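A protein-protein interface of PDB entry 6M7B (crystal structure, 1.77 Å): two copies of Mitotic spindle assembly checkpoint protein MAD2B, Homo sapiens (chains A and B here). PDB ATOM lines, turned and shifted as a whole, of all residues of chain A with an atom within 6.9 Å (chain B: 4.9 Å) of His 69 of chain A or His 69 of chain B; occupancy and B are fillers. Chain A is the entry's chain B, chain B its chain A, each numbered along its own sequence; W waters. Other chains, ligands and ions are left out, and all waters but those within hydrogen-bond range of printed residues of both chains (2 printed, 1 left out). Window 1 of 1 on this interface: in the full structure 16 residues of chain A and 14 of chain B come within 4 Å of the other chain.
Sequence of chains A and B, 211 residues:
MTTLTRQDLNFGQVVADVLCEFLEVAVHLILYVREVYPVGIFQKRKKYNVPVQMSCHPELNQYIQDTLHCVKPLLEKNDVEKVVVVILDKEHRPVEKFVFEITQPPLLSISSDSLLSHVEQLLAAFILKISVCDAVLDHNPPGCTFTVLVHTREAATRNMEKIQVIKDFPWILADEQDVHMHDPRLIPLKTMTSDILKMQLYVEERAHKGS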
ATOM      1  N   CYS A  20     -19.663  11.498  21.792  1.00  0.00           N
ATOM      2  CA  CYS A  20     -19.490  10.820  20.512  1.00  0.00           C
ATOM      3  C   CYS A  20     -18.766   9.493  20.685  1.00  0.00           C
ATOM      4  O   CYS A  20     -19.167   8.483  20.099  1.00  0.00           O
ATOM      5  CB  CYS A  20     -18.760  11.722  19.529  1.00  0.00           C
ATOM      6  SG  CYS A  20     -19.882  12.940  18.852  1.00  0.00           S
ATOM      7  N   GLU A  24     -20.717   5.873  19.978  1.00  0.00           N
ATOM      8  CA  GLU A  24     -20.193   4.886  19.046  1.00  0.00           C
ATOM      9  C   GLU A  24     -20.158   3.508  19.695  1.00  0.00           C
ATOM     10  O   GLU A  24     -20.622   2.532  19.104  1.00  0.00           O
ATOM     11  CB  GLU A  24     -18.802   5.278  18.550  1.00  0.00           C
ATOM     12  CG  GLU A  24     -18.239   4.245  17.592  1.00  0.00           C
ATOM     13  CD  GLU A  24     -16.847   4.585  17.108  1.00  0.00           C
ATOM     14  OE1 GLU A  24     -16.514   4.248  15.952  1.00  0.00           O
ATOM     15  OE2 GLU A  24     -16.093   5.195  17.885  1.00  0.00           O
ATOM     16  N   GLN A  62     -17.648   2.622   9.194  1.00  0.00           N
ATOM     17  CA  GLN A  62     -17.562   3.962   8.613  1.00  0.00           C
ATOM     18  C   GLN A  62     -18.910   4.666   8.639  1.00  0.00           C
ATOM     19  O   GLN A  62     -18.973   5.883   8.840  1.00  0.00           O
ATOM     20  CB  GLN A  62     -17.045   3.884   7.181  1.00  0.00           C
ATOM     21  CG  GLN A  62     -16.707   5.247   6.611  1.00  0.00           C
ATOM     22  CD  GLN A  62     -15.598   5.915   7.402  1.00  0.00           C
ATOM     23  OE1 GLN A  62     -14.541   5.323   7.620  1.00  0.00           O
ATOM     24  NE2 GLN A  62     -15.841   7.143   7.862  1.00  0.00           N
ATOM     25  N   ILE A  64     -21.283   4.318  10.923  1.00  0.00           N
ATOM     26  CA  ILE A  64     -21.531   4.783  12.280  1.00  0.00           C
ATOM     27  C   ILE A  64     -20.624   5.960  12.607  1.00  0.00           C
ATOM     28  O   ILE A  64     -21.060   6.953  13.200  1.00  0.00           O
ATOM     29  CB  ILE A  64     -21.355   3.619  13.272  1.00  0.00           C
ATOM     30  CG1 ILE A  64     -22.501   2.618  13.101  1.00  0.00           C
ATOM     31  CG2 ILE A  64     -21.311   4.141  14.701  1.00  0.00           C
ATOM     32  CD1 ILE A  64     -22.284   1.283  13.857  1.00  0.00           C
ATOM     33  N   GLN A  65     -19.357   5.877  12.201  1.00  0.00           N
ATOM     34  CA  GLN A  65     -18.432   6.992  12.381  1.00  0.00           C
ATOM     35  C   GLN A  65     -18.943   8.262  11.716  1.00  0.00           C
ATOM     36  O   GLN A  65     -18.952   9.334  12.331  1.00  0.00           O
ATOM     37  CB  GLN A  65     -17.070   6.635  11.802  1.00  0.00           C
ATOM     38  CG  GLN A  65     -16.177   5.866  12.724  1.00  0.00           C
ATOM     39  CD  GLN A  65     -14.724   6.089  12.363  1.00  0.00           C
ATOM     40  OE1 GLN A  65     -14.012   6.821  13.047  1.00  0.00           O
ATOM     41  NE2 GLN A  65     -14.283   5.474  11.272  1.00  0.00           N
ATOM     42  N   ASP A  66     -19.297   8.172  10.429  1.00  0.00           N
ATOM     43  CA  ASP A  66     -19.779   9.347   9.709  1.00  0.00           C
ATOM     44  C   ASP A  66     -21.009   9.927  10.392  1.00  0.00           C
ATOM     45  O   ASP A  66     -21.139  11.149  10.523  1.00  0.00           O
ATOM     46  CB  ASP A  66     -20.112   8.980   8.260  1.00  0.00           C
ATOM     47  CG  ASP A  66     -18.870   8.692   7.410  1.00  0.00           C
ATOM     48  OD1 ASP A  66     -17.741   8.993   7.846  1.00  0.00           O
ATOM     49  OD2 ASP A  66     -19.050   8.152   6.298  1.00  0.00           O
ATOM     50  N   THR A  67     -21.931   9.057  10.812  1.00  0.00           N
ATOM     51  CA  THR A  67     -23.136   9.513  11.493  1.00  0.00           C
ATOM     52  C   THR A  67     -22.787  10.358  12.711  1.00  0.00           C
ATOM     53  O   THR A  67     -23.296  11.471  12.877  1.00  0.00           O
ATOM     54  CB  THR A  67     -24.000   8.311  11.898  1.00  0.00           C
ATOM     55  OG1 THR A  67     -24.440   7.618  10.719  1.00  0.00           O
ATOM     56  CG2 THR A  67     -25.219   8.780  12.683  1.00  0.00           C
ATOM     57  N   LEU A  68     -21.887   9.862  13.565  1.00  0.00           N
ATOM     58  CA  LEU A  68     -21.581  10.581  14.796  1.00  0.00           C
ATOM     59  C   LEU A  68     -20.694  11.793  14.563  1.00  0.00           C
ATOM     60  O   LEU A  68     -20.801  12.770  15.310  1.00  0.00           O
ATOM     61  CB  LEU A  68     -20.931   9.641  15.814  1.00  0.00           C
ATOM     62  CG  LEU A  68     -21.866   8.484  16.183  1.00  0.00           C
ATOM     63  CD1 LEU A  68     -21.095   7.424  16.927  1.00  0.00           C
ATOM     64  CD2 LEU A  68     -23.053   8.962  17.008  1.00  0.00           C
ATOM     65  N   HIS A  69     -19.796  11.759  13.571  1.00  0.00           N
ATOM     66  CA  HIS A  69     -19.031  12.967  13.268  1.00  0.00           C
ATOM     67  C   HIS A  69     -19.957  14.110  12.888  1.00  0.00           C
ATOM     68  O   HIS A  69     -19.669  15.282  13.179  1.00  0.00           O
ATOM     69  CB  HIS A  69     -18.021  12.702  12.148  1.00  0.00           C
ATOM     70  CG  HIS A  69     -16.953  11.726  12.528  1.00  0.00           C
ATOM     71  ND1 HIS A  69     -16.547  11.544  13.833  1.00  0.00           N
ATOM     72  CD2 HIS A  69     -16.217  10.866  11.783  1.00  0.00           C
ATOM     73  CE1 HIS A  69     -15.606  10.617  13.877  1.00  0.00           C
ATOM     74  NE2 HIS A  69     -15.388  10.189  12.645  1.00  0.00           N
ATOM     75  N   CYS A  70     -21.088  13.781  12.267  1.00  0.00           N
ATOM     76  CA  CYS A  70     -22.049  14.805  11.878  1.00  0.00           C
ATOM     77  C   CYS A  70     -22.800  15.361  13.083  1.00  0.00           C
ATOM     78  O   CYS A  70     -23.141  16.545  13.101  1.00  0.00           O
ATOM     79  CB  CYS A  70     -23.037  14.226  10.867  1.00  0.00           C
ATOM     80  SG  CYS A  70     -22.373  13.934   9.195  1.00  0.00           S
ATOM     81  N   VAL A  71     -23.070  14.523  14.090  1.00  0.00           N
ATOM     82  CA  VAL A  71     -23.821  14.966  15.264  1.00  0.00           C
ATOM     83  C   VAL A  71     -22.949  15.808  16.191  1.00  0.00           C
ATOM     84  O   VAL A  71     -23.458  16.694  16.896  1.00  0.00           O
ATOM     85  CB  VAL A  71     -24.391  13.739  16.000  1.00  0.00           C
ATOM     86  CG1 VAL A  71     -25.216  14.150  17.208  1.00  0.00           C
ATOM     87  CG2 VAL A  71     -25.230  12.894  15.043  1.00  0.00           C
ATOM     88  N   LYS A  72     -21.631  15.572  16.175  1.00  0.00           N
ATOM     89  CA  LYS A  72     -20.709  16.215  17.116  1.00  0.00           C
ATOM     90  C   LYS A  72     -20.828  17.732  17.166  1.00  0.00           C
ATOM     91  O   LYS A  72     -20.976  18.277  18.273  1.00  0.00           O
ATOM     92  CB  LYS A  72     -19.271  15.776  16.790  1.00  0.00           C
ATOM     93  CG  LYS A  72     -18.203  16.413  17.687  1.00  0.00           C
ATOM     94  CD  LYS A  72     -17.165  15.394  18.171  1.00  0.00           C
ATOM     95  CE  LYS A  72     -16.277  14.878  17.050  1.00  0.00           C
ATOM     96  NZ  LYS A  72     -14.938  14.490  17.589  1.00  0.00           N
ATOM     97  N   PRO A  73     -20.788  18.476  16.051  1.00  0.00           N
ATOM     98  CA  PRO A  73     -20.915  19.938  16.187  1.00  0.00           C
ATOM     99  C   PRO A  73     -22.216  20.367  16.839  1.00  0.00           C
ATOM    100  O   PRO A  73     -22.233  21.370  17.566  1.00  0.00           O
ATOM    101  CB  PRO A  73     -20.807  20.447  14.740  1.00  0.00           C
ATOM    102  CG  PRO A  73     -21.193  19.288  13.904  1.00  0.00           C
ATOM    103  CD  PRO A  73     -20.691  18.071  14.636  1.00  0.00           C
ATOM    104  N   LEU A  74     -23.307  19.624  16.615  1.00  0.00           N
ATOM    105  CA  LEU A  74     -24.572  19.947  17.268  1.00  0.00           C
ATOM    106  C   LEU A  74     -24.500  19.672  18.763  1.00  0.00           C
ATOM    107  O   LEU A  74     -25.059  20.433  19.564  1.00  0.00           O
ATOM    108  CB  LEU A  74     -25.716  19.149  16.636  1.00  0.00           C
ATOM    109  CG  LEU A  74     -26.157  19.483  15.207  1.00  0.00           C
ATOM    110  CD1 LEU A  74     -27.069  18.389  14.674  1.00  0.00           C
ATOM    111  CD2 LEU A  74     -26.873  20.801  15.198  1.00  0.00           C
ATOM    112  N   LYS A 162     -25.703  22.683   9.809  1.00  0.00           N
ATOM    113  CA  LYS A 162     -24.602  22.327  10.693  1.00  0.00           C
ATOM    114  C   LYS A 162     -24.344  20.825  10.746  1.00  0.00           C
ATOM    115  O   LYS A 162     -23.215  20.419  11.044  1.00  0.00           O
ATOM    116  CB  LYS A 162     -24.868  22.902  12.086  1.00  0.00           C
ATOM    117  CG  LYS A 162     -24.858  24.436  12.070  1.00  0.00           C
ATOM    118  CD  LYS A 162     -25.188  25.088  13.407  1.00  0.00           C
ATOM    119  CE  LYS A 162     -26.437  24.506  14.055  1.00  0.00           C
ATOM    120  NZ  LYS A 162     -26.826  25.276  15.275  1.00  0.00           N
ATOM    121  N   ILE A 163     -25.346  19.992  10.452  1.00  0.00           N
ATOM    122  CA  ILE A 163     -25.167  18.545  10.556  1.00  0.00           C
ATOM    123  C   ILE A 163     -24.447  17.935   9.351  1.00  0.00           C
ATOM    124  O   ILE A 163     -23.945  16.814   9.454  1.00  0.00           O
ATOM    125  CB  ILE A 163     -26.532  17.856  10.750  1.00  0.00           C
ATOM    126  CG1 ILE A 163     -26.367  16.444  11.320  1.00  0.00           C
ATOM    127  CG2 ILE A 163     -27.293  17.788   9.438  1.00  0.00           C
ATOM    128  CD1 ILE A 163     -27.651  15.889  11.911  1.00  0.00           C
ATOM    129  N   VAL A 165     -21.649  17.495   7.917  1.00  0.00           N
ATOM    130  CA  VAL A 165     -20.222  17.664   8.176  1.00  0.00           C
ATOM    131  C   VAL A 165     -19.371  16.885   7.171  1.00  0.00           C
ATOM    132  O   VAL A 165     -18.274  17.325   6.798  1.00  0.00           O
ATOM    133  CB  VAL A 165     -19.929  17.209   9.626  1.00  0.00           C
ATOM    134  CG1 VAL A 165     -18.438  16.915   9.830  1.00  0.00           C
ATOM    135  CG2 VAL A 165     -20.414  18.251  10.613  1.00  0.00           C
ATOM    136  N   ILE A 166     -19.862  15.733   6.726  1.00  0.00           N
ATOM    137  CA  ILE A 166     -19.063  14.714   6.053  1.00  0.00           C
ATOM    138  C   ILE A 166     -19.429  14.691   4.572  1.00  0.00           C
ATOM    139  O   ILE A 166     -20.610  14.584   4.216  1.00  0.00           O
ATOM    140  CB  ILE A 166     -19.287  13.338   6.702  1.00  0.00           C
ATOM    141  CG1 ILE A 166     -18.742  13.323   8.137  1.00  0.00           C
ATOM    142  CG2 ILE A 166     -18.656  12.216   5.868  1.00  0.00           C
ATOM    143  CD1 ILE A 166     -17.262  13.578   8.226  1.00  0.00           C
ATOM    144  N   LYS A 167     -18.412  14.785   3.715  1.00  0.00           N
ATOM    145  CA  LYS A 167     -18.605  14.675   2.268  1.00  0.00           C
ATOM    146  C   LYS A 167     -19.387  13.415   1.906  1.00  0.00           C
ATOM    147  O   LYS A 167     -19.110  12.326   2.416  1.00  0.00           O
ATOM    148  CB  LYS A 167     -17.241  14.662   1.574  1.00  0.00           C
ATOM    149  CG  LYS A 167     -17.275  14.410   0.066  1.00  0.00           C
ATOM    150  CD  LYS A 167     -15.929  14.803  -0.544  1.00  0.00           C
ATOM    151  CE  LYS A 167     -15.786  14.390  -2.004  1.00  0.00           C
ATOM    152  NZ  LYS A 167     -15.609  12.920  -2.132  1.00  0.00           N
ATOM    153  N   TRP A 171     -27.900  14.308   5.162  1.00  0.00           N
ATOM    154  CA  TRP A 171     -28.985  14.059   6.103  1.00  0.00           C
ATOM    155  C   TRP A 171     -30.284  14.632   5.545  1.00  0.00           C
ATOM    156  O   TRP A 171     -30.266  15.550   4.725  1.00  0.00           O
ATOM    157  CB  TRP A 171     -28.678  14.711   7.450  1.00  0.00           C
ATOM    158  CG  TRP A 171     -27.576  14.061   8.215  1.00  0.00           C
ATOM    159  CD1 TRP A 171     -26.242  14.031   7.895  1.00  0.00           C
ATOM    160  CD2 TRP A 171     -27.713  13.344   9.442  1.00  0.00           C
ATOM    161  NE1 TRP A 171     -25.543  13.324   8.865  1.00  0.00           N
ATOM    162  CE2 TRP A 171     -26.430  12.890   9.815  1.00  0.00           C
ATOM    163  CE3 TRP A 171     -28.803  13.038  10.262  1.00  0.00           C
ATOM    164  CZ2 TRP A 171     -26.211  12.159  10.976  1.00  0.00           C
ATOM    165  CZ3 TRP A 171     -28.585  12.306  11.408  1.00  0.00           C
ATOM    166  CH2 TRP A 171     -27.300  11.874  11.755  1.00  0.00           C
ATOM    167  N   GLN B  65      -7.677  14.362  14.511  1.00  0.00           N
ATOM    168  CA  GLN B  65      -8.717  13.478  14.000  1.00  0.00           C
ATOM    169  C   GLN B  65      -9.154  13.900  12.610  1.00  0.00           C
ATOM    170  O   GLN B  65      -9.271  13.062  11.699  1.00  0.00           O
ATOM    171  CB  GLN B  65      -9.927  13.476  14.932  1.00  0.00           C
ATOM    172  CG  GLN B  65      -9.775  12.602  16.140  1.00  0.00           C
ATOM    173  CD  GLN B  65     -11.075  11.938  16.541  1.00  0.00           C
ATOM    174  OE1 GLN B  65     -12.147  12.280  16.032  1.00  0.00           O
ATOM    175  NE2 GLN B  65     -10.985  10.969  17.449  1.00  0.00           N
ATOM    176  N   ASP B  66      -9.429  15.200  12.433  1.00  0.00           N
ATOM    177  CA  ASP B  66      -9.936  15.667  11.146  1.00  0.00           C
ATOM    178  C   ASP B  66      -8.902  15.457  10.053  1.00  0.00           C
ATOM    179  O   ASP B  66      -9.247  15.119   8.914  1.00  0.00           O
ATOM    180  CB  ASP B  66     -10.298  17.157  11.179  1.00  0.00           C
ATOM    181  CG  ASP B  66     -11.593  17.460  11.929  1.00  0.00           C
ATOM    182  OD1 ASP B  66     -11.798  18.665  12.216  1.00  0.00           O
ATOM    183  OD2 ASP B  66     -12.345  16.520  12.287  1.00  0.00           O
ATOM    184  N   THR B  67      -7.634  15.719  10.374  1.00  0.00           N
ATOM    185  CA  THR B  67      -6.561  15.528   9.405  1.00  0.00           C
ATOM    186  C   THR B  67      -6.543  14.093   8.892  1.00  0.00           C
ATOM    187  O   THR B  67      -6.541  13.850   7.677  1.00  0.00           O
ATOM    188  CB  THR B  67      -5.217  15.912  10.046  1.00  0.00           C
ATOM    189  OG1 THR B  67      -5.246  17.297  10.430  1.00  0.00           O
ATOM    190  CG2 THR B  67      -4.049  15.681   9.078  1.00  0.00           C
ATOM    191  N   LEU B  68      -6.547  13.119   9.802  1.00  0.00           N
ATOM    192  CA  LEU B  68      -6.436  11.730   9.356  1.00  0.00           C
ATOM    193  C   LEU B  68      -7.729  11.232   8.732  1.00  0.00           C
ATOM    194  O   LEU B  68      -7.684  10.396   7.818  1.00  0.00           O
ATOM    195  CB  LEU B  68      -5.978  10.855  10.528  1.00  0.00           C
ATOM    196  CG  LEU B  68      -4.547  11.318  10.812  1.00  0.00           C
ATOM    197  CD1 LEU B  68      -4.093  11.048  12.221  1.00  0.00           C
ATOM    198  CD2 LEU B  68      -3.579  10.719   9.795  1.00  0.00           C
ATOM    199  N   HIS B  69      -8.888  11.732   9.187  1.00  0.00           N
ATOM    200  CA  HIS B  69     -10.144  11.390   8.531  1.00  0.00           C
ATOM    201  C   HIS B  69     -10.105  11.755   7.050  1.00  0.00           C
ATOM    202  O   HIS B  69     -10.634  11.020   6.207  1.00  0.00           O
ATOM    203  CB  HIS B  69     -11.300  12.100   9.240  1.00  0.00           C
ATOM    204  CG  HIS B  69     -12.661  11.653   8.807  1.00  0.00           C
ATOM    205  ND1 HIS B  69     -13.087  11.704   7.499  1.00  0.00           N
ATOM    206  CD2 HIS B  69     -13.705  11.173   9.523  1.00  0.00           C
ATOM    207  CE1 HIS B  69     -14.334  11.271   7.428  1.00  0.00           C
ATOM    208  NE2 HIS B  69     -14.728  10.932   8.640  1.00  0.00           N
ATOM    209  N   CYS B  70      -9.476  12.882   6.717  1.00  0.00           N
ATOM    210  CA  CYS B  70      -9.384  13.316   5.324  1.00  0.00           C
ATOM    211  C   CYS B  70      -8.429  12.440   4.526  1.00  0.00           C
ATOM    212  O   CYS B  70      -8.613  12.256   3.319  1.00  0.00           O
ATOM    213  CB  CYS B  70      -8.924  14.777   5.269  1.00  0.00           C
ATOM    214  SG  CYS B  70     -10.167  15.977   5.792  1.00  0.00           S
ATOM    215  N   VAL B  71      -7.410  11.891   5.182  1.00  0.00           N
ATOM    216  CA  VAL B  71      -6.431  11.065   4.478  1.00  0.00           C
ATOM    217  C   VAL B  71      -7.024   9.709   4.118  1.00  0.00           C
ATOM    218  O   VAL B  71      -6.594   9.066   3.144  1.00  0.00           O
ATOM    219  CB  VAL B  71      -5.162  10.943   5.354  1.00  0.00           C
ATOM    220  CG1 VAL B  71      -4.111  10.025   4.699  1.00  0.00           C
ATOM    221  CG2 VAL B  71      -4.573  12.323   5.598  1.00  0.00           C
ATOM    222  N   LYS B  72      -8.040   9.267   4.864  1.00  0.00           N
ATOM    223  CA  LYS B  72      -8.517   7.892   4.740  1.00  0.00           C
ATOM    224  C   LYS B  72      -8.926   7.504   3.325  1.00  0.00           C
ATOM    225  O   LYS B  72      -8.527   6.415   2.872  1.00  0.00           O
ATOM    226  CB  LYS B  72      -9.668   7.653   5.725  1.00  0.00           C
ATOM    227  CG  LYS B  72     -10.111   6.195   5.774  1.00  0.00           C
ATOM    228  CD  LYS B  72     -11.324   6.011   6.665  1.00  0.00           C
ATOM    229  CE  LYS B  72     -10.918   5.592   8.061  1.00  0.00           C
ATOM    230  NZ  LYS B  72     -12.103   5.339   8.932  1.00  0.00           N
ATOM    231  N   PRO B  73      -9.710   8.297   2.578  1.00  0.00           N
ATOM    232  CA  PRO B  73     -10.074   7.851   1.225  1.00  0.00           C
ATOM    233  C   PRO B  73      -8.882   7.766   0.297  1.00  0.00           C
ATOM    234  O   PRO B  73      -8.892   6.936  -0.617  1.00  0.00           O
ATOM    235  CB  PRO B  73     -11.089   8.905   0.756  1.00  0.00           C
ATOM    236  CG  PRO B  73     -10.879  10.066   1.644  1.00  0.00           C
ATOM    237  CD  PRO B  73     -10.437   9.522   2.955  1.00  0.00           C
ATOM    238  N   VAL B 165     -12.801  15.964   2.911  1.00  0.00           N
ATOM    239  CA  VAL B 165     -13.890  15.145   3.427  1.00  0.00           C
ATOM    240  C   VAL B 165     -14.702  15.867   4.498  1.00  0.00           C
ATOM    241  O   VAL B 165     -15.860  15.505   4.738  1.00  0.00           O
ATOM    242  CB  VAL B 165     -13.301  13.834   3.999  1.00  0.00           C
ATOM    243  CG1 VAL B 165     -14.353  12.999   4.697  1.00  0.00           C
ATOM    244  CG2 VAL B 165     -12.623  13.021   2.889  1.00  0.00           C
ATOM    245  N   ILE B 166     -14.120  16.858   5.172  1.00  0.00           N
ATOM    246  CA  ILE B 166     -14.713  17.452   6.365  1.00  0.00           C
ATOM    247  C   ILE B 166     -15.046  18.909   6.071  1.00  0.00           C
ATOM    248  O   ILE B 166     -14.195  19.663   5.581  1.00  0.00           O
ATOM    249  CB  ILE B 166     -13.775  17.315   7.574  1.00  0.00           C
ATOM    250  CG1 ILE B 166     -13.657  15.836   7.940  1.00  0.00           C
ATOM    251  CG2 ILE B 166     -14.305  18.107   8.782  1.00  0.00           C
ATOM    252  CD1 ILE B 166     -12.546  15.553   8.855  1.00  0.00           C
HETATM  253  O   HOH W   1     -14.217   8.220  10.217  1.00  0.00           O
HETATM  254  O   HOH W   2     -17.789  17.984   3.483  1.00  0.00           O
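The side-chain amino group of Lys 72 of chain B lies close to the side-chain amide nitrogen of Gln 65 of chain A (3.2 Å).
NZ of Lys 72 of chain B is in hydrogen-bond range of OE1 of Gln 62 of chain A (2.8 Å).
The backbone carbonyl oxygen (O) of Val 165 of chain B lies within hydrogen-bond range of the backbone NH (N) of Lys 167 of chain A.
SG of Cys 70 of chain A is in hydrogen-bond range of O of Asp 66 of chain A, at 3.3 Å.
NE2 of Gln 62 of chain A is in hydrogen-bond range of OD1 of Asp 66 of chain A (2.7 Å).
Asp 66 of chain A touches His 69 of chain B.
His 69 of chain A touches His 69 of chain B (CD2 to CD2, 3.4 Å).
Lys 72 of chain A touches Gln 65 of chain B.
O of Val 165 of chain B touches O of Val 165 of chain A, 3.7 Å away.
CA of Ile 166 of chain B touches O of Val 165 of chain A (3.6 Å).
His 69 of chain B touches Ile 166 of chain A (NE2 to CD1, 3.7 Å).
Ile 166 of chain A touches Val 165 of chain B (CA to O, 3.6 Å).
Printed residues of chain B within 4 Å of His 69 of chain A: His 69.
Of the printed residues of chain B, Val 165 of chain A touches Val 165 and Ile 166.
Printed residues of chain B within 4 Å of Lys 167 of chain A: Val 165 (2.8 Å).
Of the printed residues of chain A, His 69 of chain B touches Asp 66 (3.7 Å), His 69 (3.4 Å) and Ile 166 (3.7 Å).
The nearest printed residue of chain A that does not touch His 69 of chain B is Gln 62 of chain A (4.02 Å).
Hydrophobic or aromatic side chains of chain A within 4 Å of the printed part of chain B: His 69 and Ile 166.
Along chain A the printed residues that touch a printed residue of chain B span positions 62 to 167.
Hydrophobic or aromatic side chains of chain B within 4 Å of the printed part of chain A: His 69.
Among the printed residues, 10 pairs touch across the chains.
Asp 66 of chain A touches His 69 of chain B, but with the chains exchanged His 69 of chain A does not touch Asp 66 of chain B (6.7 Å).
His 69 of chain B touches its own counterpart, His 69 of chain A.
Val 165 of chain B touches its own counterpart, Val 165 of chain A.
Val 165 of chain A touches Ile 166 of chain B, and with the chains exchanged Ile 166 of chain A touches Val 165 of chain B.
Positions printed for both chains: 65, 66, 67, 68, 69, 70, 71, 72, 73, 165 and 166.
Of the 10 pairs that touch across the chains among the printed residues, 6 have their exchanged pair printed and touching as well.
Water W1 lies within hydrogen-bond range of NE2 of Gln 65 of chain A (2.9 Å), NE2 of Gln 62 of chain A (3.1 Å), NE2 of His 69 of chain B (3.2 Å) and NE2 of His 69 of chain A (3.3 Å).
Water W2 lies within hydrogen-bond range of N of Lys 167 of chain A (3.3 Å), O of Val 165 of chain B (3.4 Å) and O of Val 165 of chain A (3.4 Å).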
